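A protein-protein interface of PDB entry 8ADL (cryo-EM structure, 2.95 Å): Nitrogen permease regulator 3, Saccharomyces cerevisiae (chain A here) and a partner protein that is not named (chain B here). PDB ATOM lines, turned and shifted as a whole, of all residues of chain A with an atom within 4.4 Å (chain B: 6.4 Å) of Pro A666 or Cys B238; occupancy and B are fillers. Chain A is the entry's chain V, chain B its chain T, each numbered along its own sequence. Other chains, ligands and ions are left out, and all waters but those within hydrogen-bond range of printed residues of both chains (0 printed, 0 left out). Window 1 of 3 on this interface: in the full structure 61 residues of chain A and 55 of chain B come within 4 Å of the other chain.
The guanidinium group of Arg B295 sits at hydrogen-bond distance from the backbone carbonyl oxygen of Thr B236 (2.7 Å).
The side-chain sulfur (SG) of Cys B238 is in hydrogen-bond range of the side-chain hydroxyl (OG1) of Thr B236, 2.9 Å away.
OH of Tyr A862 sits at hydrogen-bond distance from N of Val A667 (2.8 Å).
The backbone NH of Ser B240 lies within hydrogen-bond range of the side-chain carboxylate of Asp B243.
Of the 9 printed residues of chain B, 4 touch a printed residue of chain A.
Of the 8 printed residues of chain A, 4 touch a printed residue of chain B.
Among the printed residues, no Asp or Glu carboxylate lies within 4 Å of a Lys or Arg side-chain nitrogen of the other chain.
Thr B236 touches Lys A663.
O of Cys B238 touches CG of Lys A663 (3.6 Å).
Lys A663 touches Asp B243 (CG to OD2, 3.4 Å).
CD1 of Leu B305 touches O of Lys A663, 3.4 Å away.
CB of Thr B236 touches O of Leu A664, 3.7 Å away.
CG of Pro A666 touches OG1 of Thr B236, at 3.6 Å.
Cys B238 touches Pro A666.
Tyr A862 touches Cys B238.
Pro A666 touches just these residues of chain B: Thr B236 and Cys B238.
Of chain A, only Lys A663 (3.6 Å), Pro A666 (3.7 Å) and Tyr A862 (3.5 Å) come within 4 Å of Cys B238.
Of the printed residues of chain B, Leu A664 touches Thr B236.
Printed residues of chain B within 4 Å of Lys A663: Thr B236 (3.3 Å), Cys B238 (3.6 Å), Asp B243 (3.4 Å) and Leu B305 (3.4 Å).
The nearest residue of chain B that does not touch Pro A666 is Thr B237 (5.8 Å).
The nearest printed residue of chain A that does not touch Cys B238 is Leu A664 (5.4 Å).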
ATOM      1  N   GLU A   3     -33.745  -4.930  -6.543  1.00  0.00           N
ATOM      2  CA  GLU A   3     -33.020  -6.072  -7.086  1.00  0.00           C
ATOM      3  C   GLU A   3     -33.984  -7.132  -7.614  1.00  0.00           C
ATOM      4  O   GLU A   3     -34.963  -7.484  -6.957  1.00  0.00           O
ATOM      5  CB  GLU A   3     -32.088  -6.675  -6.030  1.00  0.00           C
ATOM      6  CG  GLU A   3     -31.131  -7.727  -6.576  1.00  0.00           C
ATOM      7  CD  GLU A   3     -29.819  -7.134  -7.058  1.00  0.00           C
ATOM      8  OE1 GLU A   3     -29.605  -5.920  -6.859  1.00  0.00           O
ATOM      9  OE2 GLU A   3     -29.002  -7.882  -7.635  1.00  0.00           O
ATOM     10  N   LEU A   5     -32.946 -10.250  -8.431  1.00  0.00           N
ATOM     11  CA  LEU A   5     -32.558 -11.572  -7.966  1.00  0.00           C
ATOM     12  C   LEU A   5     -33.429 -11.981  -6.778  1.00  0.00           C
ATOM     13  O   LEU A   5     -33.662 -11.175  -5.871  1.00  0.00           O
ATOM     14  CB  LEU A   5     -31.087 -11.581  -7.551  1.00  0.00           C
ATOM     15  CG  LEU A   5     -30.020 -11.782  -8.629  1.00  0.00           C
ATOM     16  CD1 LEU A   5     -28.646 -11.444  -8.073  1.00  0.00           C
ATOM     17  CD2 LEU A   5     -30.044 -13.203  -9.152  1.00  0.00           C
ATOM     18  N   LYS A 663     -23.296  -6.019 -16.109  1.00  0.00           N
ATOM     19  CA  LYS A 663     -22.245  -5.745 -15.139  1.00  0.00           C
ATOM     20  C   LYS A 663     -22.615  -4.633 -14.162  1.00  0.00           C
ATOM     21  O   LYS A 663     -21.725  -4.062 -13.523  1.00  0.00           O
ATOM     22  CB  LYS A 663     -20.939  -5.404 -15.860  1.00  0.00           C
ATOM     23  CG  LYS A 663     -20.036  -6.603 -16.120  1.00  0.00           C
ATOM     24  CD  LYS A 663     -20.458  -7.372 -17.362  1.00  0.00           C
ATOM     25  CE  LYS A 663     -20.264  -6.541 -18.620  1.00  0.00           C
ATOM     26  NZ  LYS A 663     -20.641  -7.296 -19.848  1.00  0.00           N
ATOM     27  N   LEU A 664     -23.896  -4.311 -14.035  1.00  0.00           N
ATOM     28  CA  LEU A 664     -24.323  -3.363 -13.009  1.00  0.00           C
ATOM     29  C   LEU A 664     -25.475  -3.874 -12.156  1.00  0.00           C
ATOM     30  O   LEU A 664     -25.499  -3.612 -10.951  1.00  0.00           O
ATOM     31  CB  LEU A 664     -24.710  -2.022 -13.658  1.00  0.00           C
ATOM     32  CG  LEU A 664     -23.550  -1.074 -13.980  1.00  0.00           C
ATOM     33  CD1 LEU A 664     -24.063   0.275 -14.455  1.00  0.00           C
ATOM     34  CD2 LEU A 664     -22.638  -0.905 -12.773  1.00  0.00           C
ATOM     35  N   GLN A 665     -26.426  -4.590 -12.743  1.00  0.00           N
ATOM     36  CA  GLN A 665     -27.518  -5.216 -11.997  1.00  0.00           C
ATOM     37  C   GLN A 665     -27.581  -6.703 -12.332  1.00  0.00           C
ATOM     38  O   GLN A 665     -27.967  -7.070 -13.462  1.00  0.00           O
ATOM     39  CB  GLN A 665     -28.845  -4.502 -12.257  1.00  0.00           C
ATOM     40  CG  GLN A 665     -29.167  -4.170 -13.713  1.00  0.00           C
ATOM     41  CD  GLN A 665     -30.495  -3.456 -13.866  1.00  0.00           C
ATOM     42  OE1 GLN A 665     -31.228  -3.268 -12.894  1.00  0.00           O
ATOM     43  NE2 GLN A 665     -30.814  -3.053 -15.090  1.00  0.00           N
ATOM     44  N   PRO A 666     -27.159  -7.580 -11.419  1.00  0.00           N
ATOM     45  CA  PRO A 666     -27.121  -9.016 -11.729  1.00  0.00           C
ATOM     46  C   PRO A 666     -28.509  -9.604 -11.940  1.00  0.00           C
ATOM     47  O   PRO A 666     -29.472  -9.249 -11.255  1.00  0.00           O
ATOM     48  CB  PRO A 666     -26.442  -9.627 -10.497  1.00  0.00           C
ATOM     49  CG  PRO A 666     -25.707  -8.491  -9.858  1.00  0.00           C
ATOM     50  CD  PRO A 666     -26.553  -7.283 -10.112  1.00  0.00           C
ATOM     51  N   VAL A 667     -28.596 -10.513 -12.907  1.00  0.00           N
ATOM     52  CA  VAL A 667     -29.843 -11.146 -13.320  1.00  0.00           C
ATOM     53  C   VAL A 667     -29.553 -12.639 -13.417  1.00  0.00           C
ATOM     54  O   VAL A 667     -28.442 -13.030 -13.795  1.00  0.00           O
ATOM     55  CB  VAL A 667     -30.350 -10.550 -14.661  1.00  0.00           C
ATOM     56  CG1 VAL A 667     -31.417 -11.414 -15.339  1.00  0.00           C
ATOM     57  CG2 VAL A 667     -30.887  -9.137 -14.450  1.00  0.00           C
ATOM     58  N   TYR A 862     -22.693 -15.748  -9.438  1.00  0.00           N
ATOM     59  CA  TYR A 862     -22.061 -14.421  -9.497  1.00  0.00           C
ATOM     60  C   TYR A 862     -20.839 -14.242  -8.591  1.00  0.00           C
ATOM     61  O   TYR A 862     -20.060 -15.172  -8.390  1.00  0.00           O
ATOM     62  CB  TYR A 862     -23.091 -13.328  -9.198  1.00  0.00           C
ATOM     63  CG  TYR A 862     -23.989 -13.025 -10.375  1.00  0.00           C
ATOM     64  CD1 TYR A 862     -23.521 -12.260 -11.434  1.00  0.00           C
ATOM     65  CD2 TYR A 862     -25.296 -13.495 -10.429  1.00  0.00           C
ATOM     66  CE1 TYR A 862     -24.321 -11.969 -12.518  1.00  0.00           C
ATOM     67  CE2 TYR A 862     -26.110 -13.208 -11.518  1.00  0.00           C
ATOM     68  CZ  TYR A 862     -25.613 -12.443 -12.558  1.00  0.00           C
ATOM     69  OH  TYR A 862     -26.397 -12.144 -13.648  1.00  0.00           O
ATOM     70  N   THR B 236     -22.109  -3.577  -7.503  1.00  0.00           N
ATOM     71  CA  THR B 236     -22.087  -5.001  -7.789  1.00  0.00           C
ATOM     72  C   THR B 236     -20.661  -5.540  -7.690  1.00  0.00           C
ATOM     73  O   THR B 236     -19.679  -4.792  -7.657  1.00  0.00           O
ATOM     74  CB  THR B 236     -22.669  -5.281  -9.173  1.00  0.00           C
ATOM     75  OG1 THR B 236     -22.597  -6.685  -9.448  1.00  0.00           O
ATOM     76  CG2 THR B 236     -21.894  -4.521 -10.236  1.00  0.00           C
ATOM     77  N   THR B 237     -20.556  -6.865  -7.640  1.00  0.00           N
ATOM     78  CA  THR B 237     -19.272  -7.553  -7.638  1.00  0.00           C
ATOM     79  C   THR B 237     -18.936  -8.144  -9.002  1.00  0.00           C
ATOM     80  O   THR B 237     -17.967  -8.900  -9.119  1.00  0.00           O
ATOM     81  CB  THR B 237     -19.258  -8.653  -6.573  1.00  0.00           C
ATOM     82  OG1 THR B 237     -20.361  -9.542  -6.785  1.00  0.00           O
ATOM     83  CG2 THR B 237     -19.360  -8.047  -5.182  1.00  0.00           C
ATOM     84  N   CYS B 238     -19.715  -7.813 -10.031  1.00  0.00           N
ATOM     85  CA  CYS B 238     -19.541  -8.368 -11.367  1.00  0.00           C
ATOM     86  C   CYS B 238     -18.514  -7.620 -12.206  1.00  0.00           C
ATOM     87  O   CYS B 238     -18.277  -8.011 -13.355  1.00  0.00           O
ATOM     88  CB  CYS B 238     -20.882  -8.371 -12.105  1.00  0.00           C
ATOM     89  SG  CYS B 238     -22.264  -8.984 -11.123  1.00  0.00           S
ATOM     90  N   VAL B 239     -17.907  -6.557 -11.675  1.00  0.00           N
ATOM     91  CA  VAL B 239     -16.875  -5.842 -12.414  1.00  0.00           C
ATOM     92  C   VAL B 239     -15.615  -6.699 -12.489  1.00  0.00           C
ATOM     93  O   VAL B 239     -15.227  -7.364 -11.516  1.00  0.00           O
ATOM     94  CB  VAL B 239     -16.624  -4.457 -11.783  1.00  0.00           C
ATOM     95  CG1 VAL B 239     -16.142  -4.559 -10.333  1.00  0.00           C
ATOM     96  CG2 VAL B 239     -15.658  -3.634 -12.629  1.00  0.00           C
ATOM     97  N   SER B 240     -15.001  -6.744 -13.669  1.00  0.00           N
ATOM     98  CA  SER B 240     -13.871  -7.631 -13.907  1.00  0.00           C
ATOM     99  C   SER B 240     -12.812  -6.872 -14.698  1.00  0.00           C
ATOM    100  O   SER B 240     -12.921  -5.663 -14.926  1.00  0.00           O
ATOM    101  CB  SER B 240     -14.329  -8.910 -14.621  1.00  0.00           C
ATOM    102  OG  SER B 240     -15.208  -8.611 -15.691  1.00  0.00           O
ATOM    103  N   GLU B 242     -11.829  -7.330 -17.904  1.00  0.00           N
ATOM    104  CA  GLU B 242     -12.108  -7.041 -19.304  1.00  0.00           C
ATOM    105  C   GLU B 242     -13.095  -5.896 -19.494  1.00  0.00           C
ATOM    106  O   GLU B 242     -13.275  -5.439 -20.626  1.00  0.00           O
ATOM    107  CB  GLU B 242     -12.635  -8.296 -20.008  1.00  0.00           C
ATOM    108  CG  GLU B 242     -14.128  -8.539 -19.833  1.00  0.00           C
ATOM    109  CD  GLU B 242     -14.442  -9.486 -18.692  1.00  0.00           C
ATOM    110  OE1 GLU B 242     -13.577  -9.668 -17.811  1.00  0.00           O
ATOM    111  OE2 GLU B 242     -15.558 -10.048 -18.675  1.00  0.00           O
ATOM    112  N   ASP B 243     -13.741  -5.428 -18.430  1.00  0.00           N
ATOM    113  CA  ASP B 243     -14.694  -4.336 -18.553  1.00  0.00           C
ATOM    114  C   ASP B 243     -13.957  -3.008 -18.662  1.00  0.00           C
ATOM    115  O   ASP B 243     -13.006  -2.747 -17.921  1.00  0.00           O
ATOM    116  CB  ASP B 243     -15.643  -4.314 -17.355  1.00  0.00           C
ATOM    117  CG  ASP B 243     -16.416  -5.609 -17.200  1.00  0.00           C
ATOM    118  OD1 ASP B 243     -16.771  -6.218 -18.232  1.00  0.00           O
ATOM    119  OD2 ASP B 243     -16.672  -6.017 -16.048  1.00  0.00           O
ATOM    120  N   ARG B 295     -15.897   0.366  -8.310  1.00  0.00           N
ATOM    121  CA  ARG B 295     -17.108   0.082  -7.544  1.00  0.00           C
ATOM    122  C   ARG B 295     -17.580   1.304  -6.763  1.00  0.00           C
ATOM    123  O   ARG B 295     -18.783   1.577  -6.693  1.00  0.00           O
ATOM    124  CB  ARG B 295     -16.872  -1.099  -6.605  1.00  0.00           C
ATOM    125  CG  ARG B 295     -17.142  -2.448  -7.243  1.00  0.00           C
ATOM    126  CD  ARG B 295     -16.915  -3.581  -6.259  1.00  0.00           C
ATOM    127  NE  ARG B 295     -18.150  -3.956  -5.579  1.00  0.00           N
ATOM    128  CZ  ARG B 295     -18.220  -4.340  -4.312  1.00  0.00           C
ATOM    129  NH1 ARG B 295     -17.141  -4.413  -3.550  1.00  0.00           N
ATOM    130  NH2 ARG B 295     -19.404  -4.660  -3.796  1.00  0.00           N
ATOM    131  N   LEU B 305     -19.899   0.610 -16.894  1.00  0.00           N
ATOM    132  CA  LEU B 305     -18.963  -0.313 -17.518  1.00  0.00           C
ATOM    133  C   LEU B 305     -19.360  -0.618 -18.961  1.00  0.00           C
ATOM    134  O   LEU B 305     -20.524  -0.503 -19.355  1.00  0.00           O
ATOM    135  CB  LEU B 305     -18.883  -1.610 -16.715  1.00  0.00           C
ATOM    136  CG  LEU B 305     -18.445  -1.452 -15.259  1.00  0.00           C
ATOM    137  CD1 LEU B 305     -18.766  -2.705 -14.466  1.00  0.00           C
ATOM    138  CD2 LEU B 305     -16.961  -1.130 -15.184  1.00  0.00           C
